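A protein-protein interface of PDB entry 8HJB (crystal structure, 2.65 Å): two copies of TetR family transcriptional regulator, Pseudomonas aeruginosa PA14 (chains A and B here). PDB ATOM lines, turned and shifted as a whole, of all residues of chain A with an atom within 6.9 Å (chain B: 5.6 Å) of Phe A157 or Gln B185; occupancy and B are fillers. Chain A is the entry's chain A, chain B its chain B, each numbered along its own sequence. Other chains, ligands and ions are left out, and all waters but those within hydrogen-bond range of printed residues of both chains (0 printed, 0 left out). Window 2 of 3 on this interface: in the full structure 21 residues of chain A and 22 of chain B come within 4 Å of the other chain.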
ATOM      1  N   ILE A 141       2.347   6.960  22.861  1.00  0.00           N
ATOM      2  CA  ILE A 141       3.031   7.885  23.758  1.00  0.00           C
ATOM      3  C   ILE A 141       2.018   8.742  24.509  1.00  0.00           C
ATOM      4  O   ILE A 141       2.063   8.848  25.739  1.00  0.00           O
ATOM      5  CB  ILE A 141       4.039   8.746  22.979  1.00  0.00           C
ATOM      6  CG1 ILE A 141       5.011   7.857  22.203  1.00  0.00           C
ATOM      7  CG2 ILE A 141       4.789   9.655  23.929  1.00  0.00           C
ATOM      8  CD1 ILE A 141       6.296   8.552  21.800  1.00  0.00           C
ATOM      9  N   VAL A 153       5.534  14.835  29.083  1.00  0.00           N
ATOM     10  CA  VAL A 153       6.344  15.801  28.349  1.00  0.00           C
ATOM     11  C   VAL A 153       5.775  15.856  26.935  1.00  0.00           C
ATOM     12  O   VAL A 153       4.899  15.046  26.604  1.00  0.00           O
ATOM     13  CB  VAL A 153       7.831  15.409  28.347  1.00  0.00           C
ATOM     14  CG1 VAL A 153       8.485  15.778  29.676  1.00  0.00           C
ATOM     15  CG2 VAL A 153       7.999  13.930  28.027  1.00  0.00           C
ATOM     16  N   PRO A 154       6.194  16.800  26.093  1.00  0.00           N
ATOM     17  CA  PRO A 154       5.865  16.701  24.667  1.00  0.00           C
ATOM     18  C   PRO A 154       6.210  15.341  24.132  1.00  0.00           C
ATOM     19  O   PRO A 154       7.356  14.871  24.289  1.00  0.00           O
ATOM     20  CB  PRO A 154       6.739  17.795  24.027  1.00  0.00           C
ATOM     21  CG  PRO A 154       7.099  18.734  25.134  1.00  0.00           C
ATOM     22  CD  PRO A 154       6.732  18.120  26.455  1.00  0.00           C
ATOM     23  N   PRO A 155       5.265  14.632  23.510  1.00  0.00           N
ATOM     24  CA  PRO A 155       5.554  13.279  23.018  1.00  0.00           C
ATOM     25  C   PRO A 155       6.702  13.230  22.025  1.00  0.00           C
ATOM     26  O   PRO A 155       7.268  12.154  21.802  1.00  0.00           O
ATOM     27  CB  PRO A 155       4.236  12.843  22.372  1.00  0.00           C
ATOM     28  CG  PRO A 155       3.193  13.709  22.994  1.00  0.00           C
ATOM     29  CD  PRO A 155       3.859  15.020  23.282  1.00  0.00           C
ATOM     30  N   TYR A 156       7.060  14.364  21.423  1.00  0.00           N
ATOM     31  CA  TYR A 156       8.255  14.435  20.595  1.00  0.00           C
ATOM     32  C   TYR A 156       9.525  14.274  21.421  1.00  0.00           C
ATOM     33  O   TYR A 156      10.572  13.924  20.867  1.00  0.00           O
ATOM     34  CB  TYR A 156       8.268  15.759  19.831  1.00  0.00           C
ATOM     35  CG  TYR A 156       6.878  16.304  19.580  1.00  0.00           C
ATOM     36  CD1 TYR A 156       5.992  15.639  18.740  1.00  0.00           C
ATOM     37  CD2 TYR A 156       6.446  17.470  20.195  1.00  0.00           C
ATOM     38  CE1 TYR A 156       4.720  16.126  18.513  1.00  0.00           C
ATOM     39  CE2 TYR A 156       5.173  17.966  19.972  1.00  0.00           C
ATOM     40  CZ  TYR A 156       4.316  17.290  19.131  1.00  0.00           C
ATOM     41  OH  TYR A 156       3.048  17.778  18.906  1.00  0.00           O
ATOM     42  N   PHE A 157       9.452  14.524  22.730  1.00  0.00           N
ATOM     43  CA  PHE A 157      10.565  14.195  23.616  1.00  0.00           C
ATOM     44  C   PHE A 157      10.786  12.691  23.668  1.00  0.00           C
ATOM     45  O   PHE A 157      11.929  12.218  23.658  1.00  0.00           O
ATOM     46  CB  PHE A 157      10.290  14.727  25.024  1.00  0.00           C
ATOM     47  CG  PHE A 157      10.675  16.162  25.227  1.00  0.00           C
ATOM     48  CD1 PHE A 157      10.402  17.114  24.261  1.00  0.00           C
ATOM     49  CD2 PHE A 157      11.269  16.567  26.411  1.00  0.00           C
ATOM     50  CE1 PHE A 157      10.746  18.434  24.454  1.00  0.00           C
ATOM     51  CE2 PHE A 157      11.608  17.890  26.613  1.00  0.00           C
ATOM     52  CZ  PHE A 157      11.347  18.825  25.629  1.00  0.00           C
ATOM     53  N   HIS A 158       9.695  11.923  23.710  1.00  0.00           N
ATOM     54  CA  HIS A 158       9.794  10.492  23.977  1.00  0.00           C
ATOM     55  C   HIS A 158      10.321   9.729  22.766  1.00  0.00           C
ATOM     56  O   HIS A 158      11.352   9.050  22.850  1.00  0.00           O
ATOM     57  CB  HIS A 158       8.432   9.948  24.412  1.00  0.00           C
ATOM     58  CG  HIS A 158       8.136  10.147  25.866  1.00  0.00           C
ATOM     59  ND1 HIS A 158       9.014   9.775  26.863  1.00  0.00           N
ATOM     60  CD2 HIS A 158       7.056  10.670  26.494  1.00  0.00           C
ATOM     61  CE1 HIS A 158       8.489  10.065  28.040  1.00  0.00           C
ATOM     62  NE2 HIS A 158       7.302  10.608  27.844  1.00  0.00           N
ATOM     63  N   TYR A 159       9.633   9.832  21.623  1.00  0.00           N
ATOM     64  CA  TYR A 159      10.004   9.007  20.479  1.00  0.00           C
ATOM     65  C   TYR A 159      11.378   9.363  19.924  1.00  0.00           C
ATOM     66  O   TYR A 159      11.954   8.570  19.173  1.00  0.00           O
ATOM     67  CB  TYR A 159       8.927   9.077  19.380  1.00  0.00           C
ATOM     68  CG  TYR A 159       8.644  10.429  18.734  1.00  0.00           C
ATOM     69  CD1 TYR A 159       9.656  11.194  18.164  1.00  0.00           C
ATOM     70  CD2 TYR A 159       7.346  10.924  18.675  1.00  0.00           C
ATOM     71  CE1 TYR A 159       9.387  12.416  17.569  1.00  0.00           C
ATOM     72  CE2 TYR A 159       7.069  12.144  18.082  1.00  0.00           C
ATOM     73  CZ  TYR A 159       8.093  12.886  17.532  1.00  0.00           C
ATOM     74  OH  TYR A 159       7.818  14.100  16.942  1.00  0.00           O
ATOM     75  N   CYS A 160      11.913  10.535  20.271  1.00  0.00           N
ATOM     76  CA  CYS A 160      13.300  10.829  19.936  1.00  0.00           C
ATOM     77  C   CYS A 160      14.249  10.055  20.840  1.00  0.00           C
ATOM     78  O   CYS A 160      15.247   9.497  20.369  1.00  0.00           O
ATOM     79  CB  CYS A 160      13.562  12.332  20.034  1.00  0.00           C
ATOM     80  SG  CYS A 160      12.859  13.298  18.677  1.00  0.00           S
ATOM     81  N   ALA A 161      13.952  10.006  22.142  1.00  0.00           N
ATOM     82  CA  ALA A 161      14.765   9.215  23.058  1.00  0.00           C
ATOM     83  C   ALA A 161      14.652   7.726  22.763  1.00  0.00           C
ATOM     84  O   ALA A 161      15.628   6.986  22.930  1.00  0.00           O
ATOM     85  CB  ALA A 161      14.363   9.504  24.503  1.00  0.00           C
ATOM     86  N   ALA A 162      13.474   7.270  22.332  1.00  0.00           N
ATOM     87  CA  ALA A 162      13.329   5.877  21.922  1.00  0.00           C
ATOM     88  C   ALA A 162      14.160   5.584  20.679  1.00  0.00           C
ATOM     89  O   ALA A 162      14.831   4.549  20.606  1.00  0.00           O
ATOM     90  CB  ALA A 162      11.856   5.550  21.674  1.00  0.00           C
ATOM     91  N   GLU B 180      15.230  21.540  15.634  1.00  0.00           N
ATOM     92  CA  GLU B 180      14.394  21.556  16.827  1.00  0.00           C
ATOM     93  C   GLU B 180      15.187  21.279  18.099  1.00  0.00           C
ATOM     94  O   GLU B 180      15.102  22.043  19.066  1.00  0.00           O
ATOM     95  CB  GLU B 180      13.275  20.520  16.681  1.00  0.00           C
ATOM     96  CG  GLU B 180      12.028  20.796  17.505  1.00  0.00           C
ATOM     97  CD  GLU B 180      10.774  20.239  16.859  1.00  0.00           C
ATOM     98  OE1 GLU B 180      10.897  19.476  15.878  1.00  0.00           O
ATOM     99  OE2 GLU B 180       9.664  20.561  17.331  1.00  0.00           O
ATOM    100  N   VAL B 181      15.964  20.192  18.113  1.00  0.00           N
ATOM    101  CA  VAL B 181      16.544  19.697  19.356  1.00  0.00           C
ATOM    102  C   VAL B 181      17.627  20.615  19.906  1.00  0.00           C
ATOM    103  O   VAL B 181      17.898  20.583  21.111  1.00  0.00           O
ATOM    104  CB  VAL B 181      17.099  18.272  19.163  1.00  0.00           C
ATOM    105  CG1 VAL B 181      15.976  17.246  19.213  1.00  0.00           C
ATOM    106  CG2 VAL B 181      17.868  18.174  17.859  1.00  0.00           C
ATOM    107  N   LEU B 182      18.261  21.429  19.067  1.00  0.00           N
ATOM    108  CA  LEU B 182      19.280  22.353  19.557  1.00  0.00           C
ATOM    109  C   LEU B 182      18.646  23.517  20.309  1.00  0.00           C
ATOM    110  O   LEU B 182      19.317  24.216  21.071  1.00  0.00           O
ATOM    111  CB  LEU B 182      20.138  22.883  18.406  1.00  0.00           C
ATOM    112  CG  LEU B 182      21.502  22.216  18.196  1.00  0.00           C
ATOM    113  CD1 LEU B 182      22.538  22.777  19.166  1.00  0.00           C
ATOM    114  CD2 LEU B 182      21.400  20.705  18.319  1.00  0.00           C
ATOM    115  N   GLN B 185      17.052  24.686  23.687  1.00  0.00           N
ATOM    116  CA  GLN B 185      16.082  23.722  24.194  1.00  0.00           C
ATOM    117  C   GLN B 185      16.214  23.537  25.701  1.00  0.00           C
ATOM    118  O   GLN B 185      15.284  23.833  26.451  1.00  0.00           O
ATOM    119  CB  GLN B 185      16.241  22.378  23.481  1.00  0.00           C
ATOM    120  CG  GLN B 185      15.073  21.419  23.668  1.00  0.00           C
ATOM    121  CD  GLN B 185      13.727  22.112  23.781  1.00  0.00           C
ATOM    122  OE1 GLN B 185      13.332  22.881  22.904  1.00  0.00           O
ATOM    123  NE2 GLN B 185      13.019  21.847  24.873  1.00  0.00           N
ATOM    124  N   GLU B 186      17.370  23.020  26.126  1.00  0.00           N
ATOM    125  CA  GLU B 186      17.721  22.846  27.535  1.00  0.00           C
ATOM    126  C   GLU B 186      16.853  21.809  28.244  1.00  0.00           C
ATOM    127  O   GLU B 186      17.339  21.080  29.113  1.00  0.00           O
ATOM    128  CB  GLU B 186      17.647  24.185  28.276  1.00  0.00           C
ATOM    129  CG  GLU B 186      18.772  24.409  29.270  1.00  0.00           C
ATOM    130  CD  GLU B 186      19.004  25.877  29.569  1.00  0.00           C
ATOM    131  OE1 GLU B 186      18.430  26.728  28.857  1.00  0.00           O
ATOM    132  OE2 GLU B 186      19.758  26.180  30.516  1.00  0.00           O
ATOM    133  N   GLY B 187      15.572  21.734  27.889  1.00  0.00           N
ATOM    134  CA  GLY B 187      14.659  20.805  28.526  1.00  0.00           C
ATOM    135  C   GLY B 187      14.727  19.401  27.964  1.00  0.00           C
ATOM    136  O   GLY B 187      14.730  18.426  28.722  1.00  0.00           O
ATOM    137  N   PHE B 188      14.767  19.279  26.635  1.00  0.00           N
ATOM    138  CA  PHE B 188      14.979  17.968  26.031  1.00  0.00           C
ATOM    139  C   PHE B 188      16.370  17.441  26.341  1.00  0.00           C
ATOM    140  O   PHE B 188      16.556  16.227  26.482  1.00  0.00           O
ATOM    141  CB  PHE B 188      14.755  18.033  24.521  1.00  0.00           C
ATOM    142  CG  PHE B 188      14.990  16.727  23.818  1.00  0.00           C
ATOM    143  CD1 PHE B 188      14.050  15.712  23.882  1.00  0.00           C
ATOM    144  CD2 PHE B 188      16.152  16.513  23.094  1.00  0.00           C
ATOM    145  CE1 PHE B 188      14.263  14.508  23.237  1.00  0.00           C
ATOM    146  CE2 PHE B 188      16.371  15.311  22.448  1.00  0.00           C
ATOM    147  CZ  PHE B 188      15.426  14.308  22.519  1.00  0.00           C
ATOM    148  N   PHE B 189      17.355  18.336  26.444  1.00  0.00           N
ATOM    149  CA  PHE B 189      18.668  17.937  26.930  1.00  0.00           C
ATOM    150  C   PHE B 189      18.568  17.382  28.345  1.00  0.00           C
ATOM    151  O   PHE B 189      19.023  16.267  28.622  1.00  0.00           O
ATOM    152  CB  PHE B 189      19.627  19.125  26.872  1.00  0.00           C
ATOM    153  CG  PHE B 189      21.061  18.760  27.107  1.00  0.00           C
ATOM    154  CD1 PHE B 189      21.644  17.716  26.411  1.00  0.00           C
ATOM    155  CD2 PHE B 189      21.834  19.472  28.007  1.00  0.00           C
ATOM    156  CE1 PHE B 189      22.964  17.379  26.620  1.00  0.00           C
ATOM    157  CE2 PHE B 189      23.159  19.144  28.216  1.00  0.00           C
ATOM    158  CZ  PHE B 189      23.724  18.091  27.525  1.00  0.00           C
ATOM    159  N   PHE B 191      15.985  16.247  29.638  1.00  0.00           N
ATOM    160  CA  PHE B 191      15.165  15.043  29.589  1.00  0.00           C
ATOM    161  C   PHE B 191      16.024  13.808  29.343  1.00  0.00           C
ATOM    162  O   PHE B 191      15.868  12.793  30.030  1.00  0.00           O
ATOM    163  CB  PHE B 191      14.089  15.191  28.509  1.00  0.00           C
ATOM    164  CG  PHE B 191      13.192  13.990  28.366  1.00  0.00           C
ATOM    165  CD1 PHE B 191      12.589  13.422  29.476  1.00  0.00           C
ATOM    166  CD2 PHE B 191      12.923  13.455  27.117  1.00  0.00           C
ATOM    167  CE1 PHE B 191      11.756  12.325  29.344  1.00  0.00           C
ATOM    168  CE2 PHE B 191      12.090  12.363  26.979  1.00  0.00           C
ATOM    169  CZ  PHE B 191      11.505  11.797  28.093  1.00  0.00           C
ATOM    170  N   LEU B 192      16.952  13.893  28.383  1.00  0.00           N
ATOM    171  CA  LEU B 192      17.832  12.769  28.079  1.00  0.00           C
ATOM    172  C   LEU B 192      18.669  12.370  29.288  1.00  0.00           C
ATOM    173  O   LEU B 192      18.912  11.180  29.520  1.00  0.00           O
ATOM    174  CB  LEU B 192      18.746  13.123  26.905  1.00  0.00           C
ATOM    175  CG  LEU B 192      18.105  13.487  25.567  1.00  0.00           C
ATOM    176  CD1 LEU B 192      19.181  13.764  24.530  1.00  0.00           C
ATOM    177  CD2 LEU B 192      17.174  12.381  25.098  1.00  0.00           C
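Hydrophobic or aromatic side chains of chain B within 4 Å of the printed part of chain A: Phe B188 and Phe B191. Of the 11 printed residues of chain A, 3 touch a printed residue of chain B. Hydrophobic or aromatic side chains of chain A within 4 Å of the printed part of chain B: Phe A157 and His A158. Among the printed residues, 6 pairs touch across the chains. Among the printed residues, no Asp or Glu carboxylate lies within 4 Å of a Lys or Arg side-chain nitrogen of the other chain.
No position is printed for both chains.
Phe A157 touches just these residues of chain B: Gln B185 (3.5 Å), Gly B187 (3.7 Å), Phe B188 (3.3 Å) and Phe B191 (3.3 Å). Of chain A, only Phe A157 comes within 4 Å of Gln B185. Of the printed residues of chain A, Phe B191 touches Phe A157 (3.3 Å) and His A158 (3.4 Å). Of the printed residues of chain B, Cys A160 touches Phe B188 (3.7 Å). Of the printed residues of chain B, His A158 touches Phe B191 (3.4 Å). Val B181 touches none of the printed residues of chain A. Ile A141 touches none of the printed residues of chain B. The nearest residue of chain A that does not touch Gln B185 is Pro A154 (6.7 Å).
The backbone carbonyl oxygen of Tyr A156 sits at hydrogen-bond distance from the side-chain sulfur of Cys A160 (3.2 Å).
CZ of Phe A157 touches NE2 of Gln B185 (3.5 Å). CE2 of Phe A157 touches C of Gly B187, at 3.7 Å. O of Phe A157 touches CE1 of Phe B188 (3.3 Å). Phe B191 touches Phe A157. His A158 touches Phe B191 (ND1 to CZ, 3.4 Å). Cys A160 touches Phe B188.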
